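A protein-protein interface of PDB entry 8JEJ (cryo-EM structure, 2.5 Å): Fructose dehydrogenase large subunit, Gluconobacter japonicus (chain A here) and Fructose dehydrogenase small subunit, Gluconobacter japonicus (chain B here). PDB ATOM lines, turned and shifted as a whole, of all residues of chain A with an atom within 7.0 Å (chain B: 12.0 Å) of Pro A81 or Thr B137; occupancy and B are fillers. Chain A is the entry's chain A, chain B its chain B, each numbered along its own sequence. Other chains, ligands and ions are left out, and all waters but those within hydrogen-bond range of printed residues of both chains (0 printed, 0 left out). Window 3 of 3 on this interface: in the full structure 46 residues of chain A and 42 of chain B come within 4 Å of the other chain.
ND2 of Asn A53 sits at hydrogen-bond distance from O of Val B141.
The side-chain amide oxygen of Asn A58 sits close to the side-chain carboxylate of Asp A63.
O of Phe A80 sits close to OD1 of Asn A78 (2.7 Å).
Met A54 touches Val B141 (O to CG2, 3.8 Å).
Pro A55 touches Glu B136 (CG to O, 3.7 Å).
O of Thr B137 touches CD of Pro A55 (3.5 Å).
CG of Pro A55 touches O of Ala B139, 3.6 Å away.
CG2 of Val B141 touches CA of Pro A55, 3.8 Å away.
CB of Thr B137 touches OD1 of Asn A58, 3.3 Å away.
Phe A80 touches Thr B137 (CB to CG2, 3.98 Å).
Pro A81 touches Thr B137 (CD to OG1, 3.6 Å).
Of the printed residues of chain B, Asn A53 touches Val B141 (3.2 Å).
Of the printed residues of chain B, Pro A55 touches Glu B136 (3.7 Å), Thr B137 (3.5 Å), Ala B139 (3.6 Å) and Val B141 (3.8 Å).
Of the printed residues of chain B, Asn A58 touches Thr B137 (3.3 Å).
Asn A78 touches none of the printed residues of chain B.
Of chain B, only Thr B137 comes within 4 Å of Pro A81.
Of chain A, only Pro A55, Asn A58, Phe A80 and Pro A81 come within 4 Å of Thr B137.
Of the printed residues of chain A, Ala B139 touches Pro A55 (3.6 Å).
Printed residues of chain A within 4 Å of Val B141: Asn A53 (3.2 Å), Met A54 (3.8 Å) and Pro A55 (3.8 Å).
The nearest residue of chain B that does not touch Pro A81 is Asn B138 (6.8 Å).
Printed residues of chain A that touch a printed residue of chain B: Asn A53, Met A54, Pro A55, Asn A58, Phe A80 and Pro A81.
Hydrophobic or aromatic side chains of chain A that line the printed part of chain B: Pro A55, Phe A80 and Pro A81.
Along chain A the printed residues that touch a printed residue of chain B span positions 53 to 81.
Among the printed residues, no Asp or Glu carboxylate lies within 4 Å of a Lys or Arg side-chain nitrogen of the other chain.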
ATOM      1  N   ASN A  53     -30.716 -21.145  -5.509  1.00  0.00           N
ATOM      2  CA  ASN A  53     -30.458 -22.505  -5.061  1.00  0.00           C
ATOM      3  C   ASN A  53     -28.981 -22.866  -5.111  1.00  0.00           C
ATOM      4  O   ASN A  53     -28.633 -24.037  -4.941  1.00  0.00           O
ATOM      5  CB  ASN A  53     -31.273 -23.494  -5.894  1.00  0.00           C
ATOM      6  CG  ASN A  53     -32.664 -23.703  -5.341  1.00  0.00           C
ATOM      7  OD1 ASN A  53     -33.573 -22.917  -5.605  1.00  0.00           O
ATOM      8  ND2 ASN A  53     -32.838 -24.760  -4.562  1.00  0.00           N
ATOM      9  N   MET A  54     -28.116 -21.894  -5.368  1.00  0.00           N
ATOM     10  CA  MET A  54     -26.674 -22.046  -5.273  1.00  0.00           C
ATOM     11  C   MET A  54     -26.244 -21.965  -3.808  1.00  0.00           C
ATOM     12  O   MET A  54     -26.782 -21.153  -3.052  1.00  0.00           O
ATOM     13  CB  MET A  54     -25.979 -20.966  -6.098  1.00  0.00           C
ATOM     14  CG  MET A  54     -24.596 -21.325  -6.608  1.00  0.00           C
ATOM     15  SD  MET A  54     -23.672 -19.860  -7.095  1.00  0.00           S
ATOM     16  CE  MET A  54     -24.174 -18.719  -5.819  1.00  0.00           C
ATOM     17  N   PRO A  55     -25.292 -22.796  -3.384  1.00  0.00           N
ATOM     18  CA  PRO A  55     -24.984 -22.886  -1.959  1.00  0.00           C
ATOM     19  C   PRO A  55     -24.494 -21.561  -1.411  1.00  0.00           C
ATOM     20  O   PRO A  55     -23.875 -20.757  -2.133  1.00  0.00           O
ATOM     21  CB  PRO A  55     -23.888 -23.959  -1.904  1.00  0.00           C
ATOM     22  CG  PRO A  55     -24.159 -24.808  -3.085  1.00  0.00           C
ATOM     23  CD  PRO A  55     -24.638 -23.869  -4.153  1.00  0.00           C
ATOM     24  N   ASN A  58     -20.965 -20.528  -1.980  1.00  0.00           N
ATOM     25  CA  ASN A  58     -20.762 -20.016  -3.326  1.00  0.00           C
ATOM     26  C   ASN A  58     -21.283 -18.594  -3.483  1.00  0.00           C
ATOM     27  O   ASN A  58     -20.935 -17.926  -4.458  1.00  0.00           O
ATOM     28  CB  ASN A  58     -21.437 -20.937  -4.343  1.00  0.00           C
ATOM     29  CG  ASN A  58     -20.719 -22.263  -4.501  1.00  0.00           C
ATOM     30  OD1 ASN A  58     -20.273 -22.610  -5.592  1.00  0.00           O
ATOM     31  ND2 ASN A  58     -20.613 -23.017  -3.413  1.00  0.00           N
ATOM     32  N   ASP A  63     -19.078 -16.380  -6.570  1.00  0.00           N
ATOM     33  CA  ASP A  63     -19.283 -17.306  -7.679  1.00  0.00           C
ATOM     34  C   ASP A  63     -20.297 -16.697  -8.638  1.00  0.00           C
ATOM     35  O   ASP A  63     -21.489 -16.614  -8.325  1.00  0.00           O
ATOM     36  CB  ASP A  63     -19.760 -18.660  -7.158  1.00  0.00           C
ATOM     37  CG  ASP A  63     -19.870 -19.710  -8.246  1.00  0.00           C
ATOM     38  OD1 ASP A  63     -19.538 -19.421  -9.413  1.00  0.00           O
ATOM     39  OD2 ASP A  63     -20.286 -20.840  -7.926  1.00  0.00           O
ATOM     40  N   THR A  66     -21.656 -20.275 -11.795  1.00  0.00           N
ATOM     41  CA  THR A  66     -22.495 -21.446 -11.551  1.00  0.00           C
ATOM     42  C   THR A  66     -23.954 -21.259 -11.964  1.00  0.00           C
ATOM     43  O   THR A  66     -24.526 -22.210 -12.526  1.00  0.00           O
ATOM     44  CB  THR A  66     -22.395 -21.858 -10.077  1.00  0.00           C
ATOM     45  OG1 THR A  66     -21.039 -22.196  -9.770  1.00  0.00           O
ATOM     46  CG2 THR A  66     -23.275 -23.061  -9.794  1.00  0.00           C
ATOM     47  N   ASN A  78     -15.481 -21.554 -15.148  1.00  0.00           N
ATOM     48  CA  ASN A  78     -16.005 -21.740 -13.804  1.00  0.00           C
ATOM     49  C   ASN A  78     -14.813 -21.933 -12.881  1.00  0.00           C
ATOM     50  O   ASN A  78     -13.874 -22.655 -13.224  1.00  0.00           O
ATOM     51  CB  ASN A  78     -16.949 -22.949 -13.724  1.00  0.00           C
ATOM     52  CG  ASN A  78     -18.113 -22.726 -12.775  1.00  0.00           C
ATOM     53  OD1 ASN A  78     -17.927 -22.544 -11.574  1.00  0.00           O
ATOM     54  ND2 ASN A  78     -19.325 -22.747 -13.314  1.00  0.00           N
ATOM     55  N   TYR A  79     -14.838 -21.272 -11.723  1.00  0.00           N
ATOM     56  CA  TYR A  79     -13.701 -21.296 -10.816  1.00  0.00           C
ATOM     57  C   TYR A  79     -14.006 -21.883  -9.449  1.00  0.00           C
ATOM     58  O   TYR A  79     -13.072 -22.285  -8.753  1.00  0.00           O
ATOM     59  CB  TYR A  79     -13.114 -19.887 -10.667  1.00  0.00           C
ATOM     60  CG  TYR A  79     -12.647 -19.369 -12.000  1.00  0.00           C
ATOM     61  CD1 TYR A  79     -11.367 -19.638 -12.456  1.00  0.00           C
ATOM     62  CD2 TYR A  79     -13.499 -18.646 -12.821  1.00  0.00           C
ATOM     63  CE1 TYR A  79     -10.943 -19.186 -13.680  1.00  0.00           C
ATOM     64  CE2 TYR A  79     -13.081 -18.188 -14.045  1.00  0.00           C
ATOM     65  CZ  TYR A  79     -11.802 -18.460 -14.470  1.00  0.00           C
ATOM     66  OH  TYR A  79     -11.377 -18.006 -15.695  1.00  0.00           O
ATOM     67  N   PHE A  80     -15.243 -21.931  -9.051  1.00  0.00           N
ATOM     68  CA  PHE A  80     -15.658 -22.979  -8.147  1.00  0.00           C
ATOM     69  C   PHE A  80     -15.797 -24.227  -9.012  1.00  0.00           C
ATOM     70  O   PHE A  80     -16.217 -24.130 -10.174  1.00  0.00           O
ATOM     71  CB  PHE A  80     -16.949 -22.588  -7.453  1.00  0.00           C
ATOM     72  CG  PHE A  80     -16.800 -21.342  -6.599  1.00  0.00           C
ATOM     73  CD1 PHE A  80     -16.537 -20.105  -7.186  1.00  0.00           C
ATOM     74  CD2 PHE A  80     -16.866 -21.413  -5.224  1.00  0.00           C
ATOM     75  CE1 PHE A  80     -16.378 -18.978  -6.422  1.00  0.00           C
ATOM     76  CE2 PHE A  80     -16.708 -20.282  -4.454  1.00  0.00           C
ATOM     77  CZ  PHE A  80     -16.465 -19.065  -5.056  1.00  0.00           C
ATOM     78  N   PRO A  81     -15.491 -25.415  -8.475  1.00  0.00           N
ATOM     79  CA  PRO A  81     -14.230 -26.066  -8.872  1.00  0.00           C
ATOM     80  C   PRO A  81     -13.843 -25.778 -10.307  1.00  0.00           C
ATOM     81  O   PRO A  81     -14.629 -25.947 -11.244  1.00  0.00           O
ATOM     82  CB  PRO A  81     -14.515 -27.555  -8.614  1.00  0.00           C
ATOM     83  CG  PRO A  81     -15.905 -27.716  -9.059  1.00  0.00           C
ATOM     84  CD  PRO A  81     -16.614 -26.303  -8.855  1.00  0.00           C
ATOM     85  N   ASP A  82     -12.610 -25.307 -10.464  1.00  0.00           N
ATOM     86  CA  ASP A  82     -12.112 -24.865 -11.760  1.00  0.00           C
ATOM     87  C   ASP A  82     -12.322 -25.936 -12.823  1.00  0.00           C
ATOM     88  O   ASP A  82     -11.912 -27.087 -12.655  1.00  0.00           O
ATOM     89  CB  ASP A  82     -10.626 -24.515 -11.647  1.00  0.00           C
ATOM     90  CG  ASP A  82     -10.122 -23.687 -12.813  1.00  0.00           C
ATOM     91  OD1 ASP A  82     -10.793 -23.648 -13.863  1.00  0.00           O
ATOM     92  OD2 ASP A  82      -9.043 -23.075 -12.675  1.00  0.00           O
ATOM     93  N   ASN A  83     -12.967 -25.547 -13.920  1.00  0.00           N
ATOM     94  CA  ASN A  83     -13.287 -26.465 -15.003  1.00  0.00           C
ATOM     95  C   ASN A  83     -12.202 -26.527 -16.069  1.00  0.00           C
ATOM     96  O   ASN A  83     -12.357 -27.272 -17.041  1.00  0.00           O
ATOM     97  CB  ASN A  83     -14.626 -26.081 -15.641  1.00  0.00           C
ATOM     98  CG  ASN A  83     -14.614 -24.691 -16.237  1.00  0.00           C
ATOM     99  OD1 ASN A  83     -13.747 -23.877 -15.929  1.00  0.00           O
ATOM    100  ND2 ASN A  83     -15.583 -24.411 -17.098  1.00  0.00           N
ATOM    101  N   ASN A  84     -11.123 -25.756 -15.916  1.00  0.00           N
ATOM    102  CA  ASN A  84      -9.938 -25.859 -16.768  1.00  0.00           C
ATOM    103  C   ASN A  84     -10.258 -25.525 -18.229  1.00  0.00           C
ATOM    104  O   ASN A  84      -9.607 -26.002 -19.158  1.00  0.00           O
ATOM    105  CB  ASN A  84      -9.301 -27.254 -16.616  1.00  0.00           C
ATOM    106  CG  ASN A  84      -8.100 -27.478 -17.522  1.00  0.00           C
ATOM    107  OD1 ASN A  84      -8.181 -28.220 -18.502  1.00  0.00           O
ATOM    108  ND2 ASN A  84      -6.986 -26.828 -17.209  1.00  0.00           N
ATOM    109  N   ARG B 126     -26.452 -25.866  11.750  1.00  0.00           N
ATOM    110  CA  ARG B 126     -25.878 -25.383  10.501  1.00  0.00           C
ATOM    111  C   ARG B 126     -26.852 -25.539   9.344  1.00  0.00           C
ATOM    112  O   ARG B 126     -26.920 -24.678   8.464  1.00  0.00           O
ATOM    113  CB  ARG B 126     -24.585 -26.135  10.205  1.00  0.00           C
ATOM    114  CG  ARG B 126     -23.499 -25.294   9.584  1.00  0.00           C
ATOM    115  CD  ARG B 126     -22.570 -26.166   8.766  1.00  0.00           C
ATOM    116  NE  ARG B 126     -21.986 -25.448   7.642  1.00  0.00           N
ATOM    117  CZ  ARG B 126     -20.950 -24.628   7.743  1.00  0.00           C
ATOM    118  NH1 ARG B 126     -20.385 -24.370   8.910  1.00  0.00           N
ATOM    119  NH2 ARG B 126     -20.466 -24.057   6.646  1.00  0.00           N
ATOM    120  N   GLY B 131     -29.073 -23.398   5.267  1.00  0.00           N
ATOM    121  CA  GLY B 131     -29.914 -23.944   4.226  1.00  0.00           C
ATOM    122  C   GLY B 131     -29.309 -25.097   3.457  1.00  0.00           C
ATOM    123  O   GLY B 131     -29.933 -25.574   2.502  1.00  0.00           O
ATOM    124  N   VAL B 132     -28.115 -25.554   3.835  1.00  0.00           N
ATOM    125  CA  VAL B 132     -27.456 -26.680   3.188  1.00  0.00           C
ATOM    126  C   VAL B 132     -26.969 -27.646   4.257  1.00  0.00           C
ATOM    127  O   VAL B 132     -26.829 -27.299   5.431  1.00  0.00           O
ATOM    128  CB  VAL B 132     -26.274 -26.247   2.293  1.00  0.00           C
ATOM    129  CG1 VAL B 132     -26.765 -25.433   1.118  1.00  0.00           C
ATOM    130  CG2 VAL B 132     -25.247 -25.473   3.101  1.00  0.00           C
ATOM    131  N   ILE B 133     -26.703 -28.875   3.826  1.00  0.00           N
ATOM    132  CA  ILE B 133     -26.185 -29.918   4.695  1.00  0.00           C
ATOM    133  C   ILE B 133     -24.754 -30.296   4.331  1.00  0.00           C
ATOM    134  O   ILE B 133     -23.933 -30.555   5.214  1.00  0.00           O
ATOM    135  CB  ILE B 133     -27.115 -31.152   4.668  1.00  0.00           C
ATOM    136  CG1 ILE B 133     -28.306 -30.932   5.599  1.00  0.00           C
ATOM    137  CG2 ILE B 133     -26.375 -32.410   5.069  1.00  0.00           C
ATOM    138  CD1 ILE B 133     -29.610 -31.424   5.039  1.00  0.00           C
ATOM    139  N   GLU B 134     -24.428 -30.303   3.042  1.00  0.00           N
ATOM    140  CA  GLU B 134     -23.102 -30.687   2.583  1.00  0.00           C
ATOM    141  C   GLU B 134     -22.197 -29.460   2.508  1.00  0.00           C
ATOM    142  O   GLU B 134     -22.537 -28.374   2.985  1.00  0.00           O
ATOM    143  CB  GLU B 134     -23.198 -31.405   1.238  1.00  0.00           C
ATOM    144  CG  GLU B 134     -24.409 -32.311   1.099  1.00  0.00           C
ATOM    145  CD  GLU B 134     -24.183 -33.688   1.691  1.00  0.00           C
ATOM    146  OE1 GLU B 134     -23.522 -33.791   2.746  1.00  0.00           O
ATOM    147  OE2 GLU B 134     -24.670 -34.673   1.099  1.00  0.00           O
ATOM    148  N   ASP B 135     -21.019 -29.626   1.899  1.00  0.00           N
ATOM    149  CA  ASP B 135     -20.028 -28.560   1.810  1.00  0.00           C
ATOM    150  C   ASP B 135     -19.478 -28.403   0.397  1.00  0.00           C
ATOM    151  O   ASP B 135     -18.403 -27.822   0.219  1.00  0.00           O
ATOM    152  CB  ASP B 135     -18.882 -28.808   2.793  1.00  0.00           C
ATOM    153  CG  ASP B 135     -19.169 -28.254   4.173  1.00  0.00           C
ATOM    154  OD1 ASP B 135     -19.704 -27.129   4.260  1.00  0.00           O
ATOM    155  OD2 ASP B 135     -18.863 -28.942   5.169  1.00  0.00           O
ATOM    156  N   GLU B 136     -20.187 -28.902  -0.607  1.00  0.00           N
ATOM    157  CA  GLU B 136     -19.755 -28.810  -1.992  1.00  0.00           C
ATOM    158  C   GLU B 136     -20.461 -27.657  -2.697  1.00  0.00           C
ATOM    159  O   GLU B 136     -21.400 -27.052  -2.177  1.00  0.00           O
ATOM    160  CB  GLU B 136     -20.017 -30.127  -2.727  1.00  0.00           C
ATOM    161  CG  GLU B 136     -19.110 -31.270  -2.300  1.00  0.00           C
ATOM    162  CD  GLU B 136     -19.517 -31.874  -0.972  1.00  0.00           C
ATOM    163  OE1 GLU B 136     -18.642 -32.030  -0.095  1.00  0.00           O
ATOM    164  OE2 GLU B 136     -20.712 -32.195  -0.803  1.00  0.00           O
ATOM    165  N   THR B 137     -19.983 -27.350  -3.902  1.00  0.00           N
ATOM    166  CA  THR B 137     -20.611 -26.329  -4.728  1.00  0.00           C
ATOM    167  C   THR B 137     -21.882 -26.821  -5.405  1.00  0.00           C
ATOM    168  O   THR B 137     -22.602 -26.012  -5.998  1.00  0.00           O
ATOM    169  CB  THR B 137     -19.628 -25.828  -5.789  1.00  0.00           C
ATOM    170  OG1 THR B 137     -19.496 -26.811  -6.822  1.00  0.00           O
ATOM    171  CG2 THR B 137     -18.263 -25.566  -5.169  1.00  0.00           C
ATOM    172  N   ASN B 138     -22.166 -28.122  -5.335  1.00  0.00           N
ATOM    173  CA  ASN B 138     -23.392 -28.700  -5.869  1.00  0.00           C
ATOM    174  C   ASN B 138     -24.303 -29.224  -4.765  1.00  0.00           C
ATOM    175  O   ASN B 138     -25.225 -29.999  -5.040  1.00  0.00           O
ATOM    176  CB  ASN B 138     -23.061 -29.816  -6.861  1.00  0.00           C
ATOM    177  CG  ASN B 138     -24.158 -30.032  -7.886  1.00  0.00           C
ATOM    178  OD1 ASN B 138     -24.669 -29.078  -8.472  1.00  0.00           O
ATOM    179  ND2 ASN B 138     -24.526 -31.289  -8.105  1.00  0.00           N
ATOM    180  N   ALA B 139     -24.054 -28.827  -3.519  1.00  0.00           N
ATOM    181  CA  ALA B 139     -24.909 -29.246  -2.418  1.00  0.00           C
ATOM    182  C   ALA B 139     -26.318 -28.700  -2.608  1.00  0.00           C
ATOM    183  O   ALA B 139     -26.510 -27.575  -3.074  1.00  0.00           O
ATOM    184  CB  ALA B 139     -24.334 -28.770  -1.085  1.00  0.00           C
ATOM    185  N   LYS B 140     -27.307 -29.516  -2.256  1.00  0.00           N
ATOM    186  CA  LYS B 140     -28.695 -29.106  -2.392  1.00  0.00           C
ATOM    187  C   LYS B 140     -29.039 -28.036  -1.365  1.00  0.00           C
ATOM    188  O   LYS B 140     -28.675 -28.137  -0.190  1.00  0.00           O
ATOM    189  CB  LYS B 140     -29.621 -30.308  -2.232  1.00  0.00           C
ATOM    190  CG  LYS B 140     -29.526 -31.303  -3.370  1.00  0.00           C
ATOM    191  CD  LYS B 140     -30.831 -32.049  -3.564  1.00  0.00           C
ATOM    192  CE  LYS B 140     -30.601 -33.369  -4.281  1.00  0.00           C
ATOM    193  NZ  LYS B 140     -30.137 -34.435  -3.350  1.00  0.00           N
ATOM    194  N   VAL B 141     -29.742 -27.005  -1.818  1.00  0.00           N
ATOM    195  CA  VAL B 141     -30.194 -25.916  -0.963  1.00  0.00           C
ATOM    196  C   VAL B 141     -31.649 -26.170  -0.602  1.00  0.00           C
ATOM    197  O   VAL B 141     -32.491 -26.367  -1.485  1.00  0.00           O
ATOM    198  CB  VAL B 141     -30.020 -24.553  -1.655  1.00  0.00           C
ATOM    199  CG1 VAL B 141     -30.748 -23.464  -0.887  1.00  0.00           C
ATOM    200  CG2 VAL B 141     -28.546 -24.216  -1.785  1.00  0.00           C
ATOM    201  N   TYR B 142     -31.944 -26.182   0.699  1.00  0.00           N
ATOM    202  CA  TYR B 142     -33.291 -26.448   1.177  1.00  0.00           C
ATOM    203  C   TYR B 142     -34.013 -25.212   1.683  1.00  0.00           C
ATOM    204  O   TYR B 142     -35.235 -25.259   1.850  1.00  0.00           O
ATOM    205  CB  TYR B 142     -33.257 -27.508   2.289  1.00  0.00           C
ATOM    206  CG  TYR B 142     -32.644 -28.806   1.826  1.00  0.00           C
ATOM    207  CD1 TYR B 142     -33.369 -29.697   1.049  1.00  0.00           C
ATOM    208  CD2 TYR B 142     -31.329 -29.127   2.138  1.00  0.00           C
ATOM    209  CE1 TYR B 142     -32.812 -30.877   0.611  1.00  0.00           C
ATOM    210  CE2 TYR B 142     -30.763 -30.307   1.704  1.00  0.00           C
ATOM    211  CZ  TYR B 142     -31.509 -31.177   0.940  1.00  0.00           C
ATOM    212  OH  TYR B 142     -30.953 -32.355   0.502  1.00  0.00           O
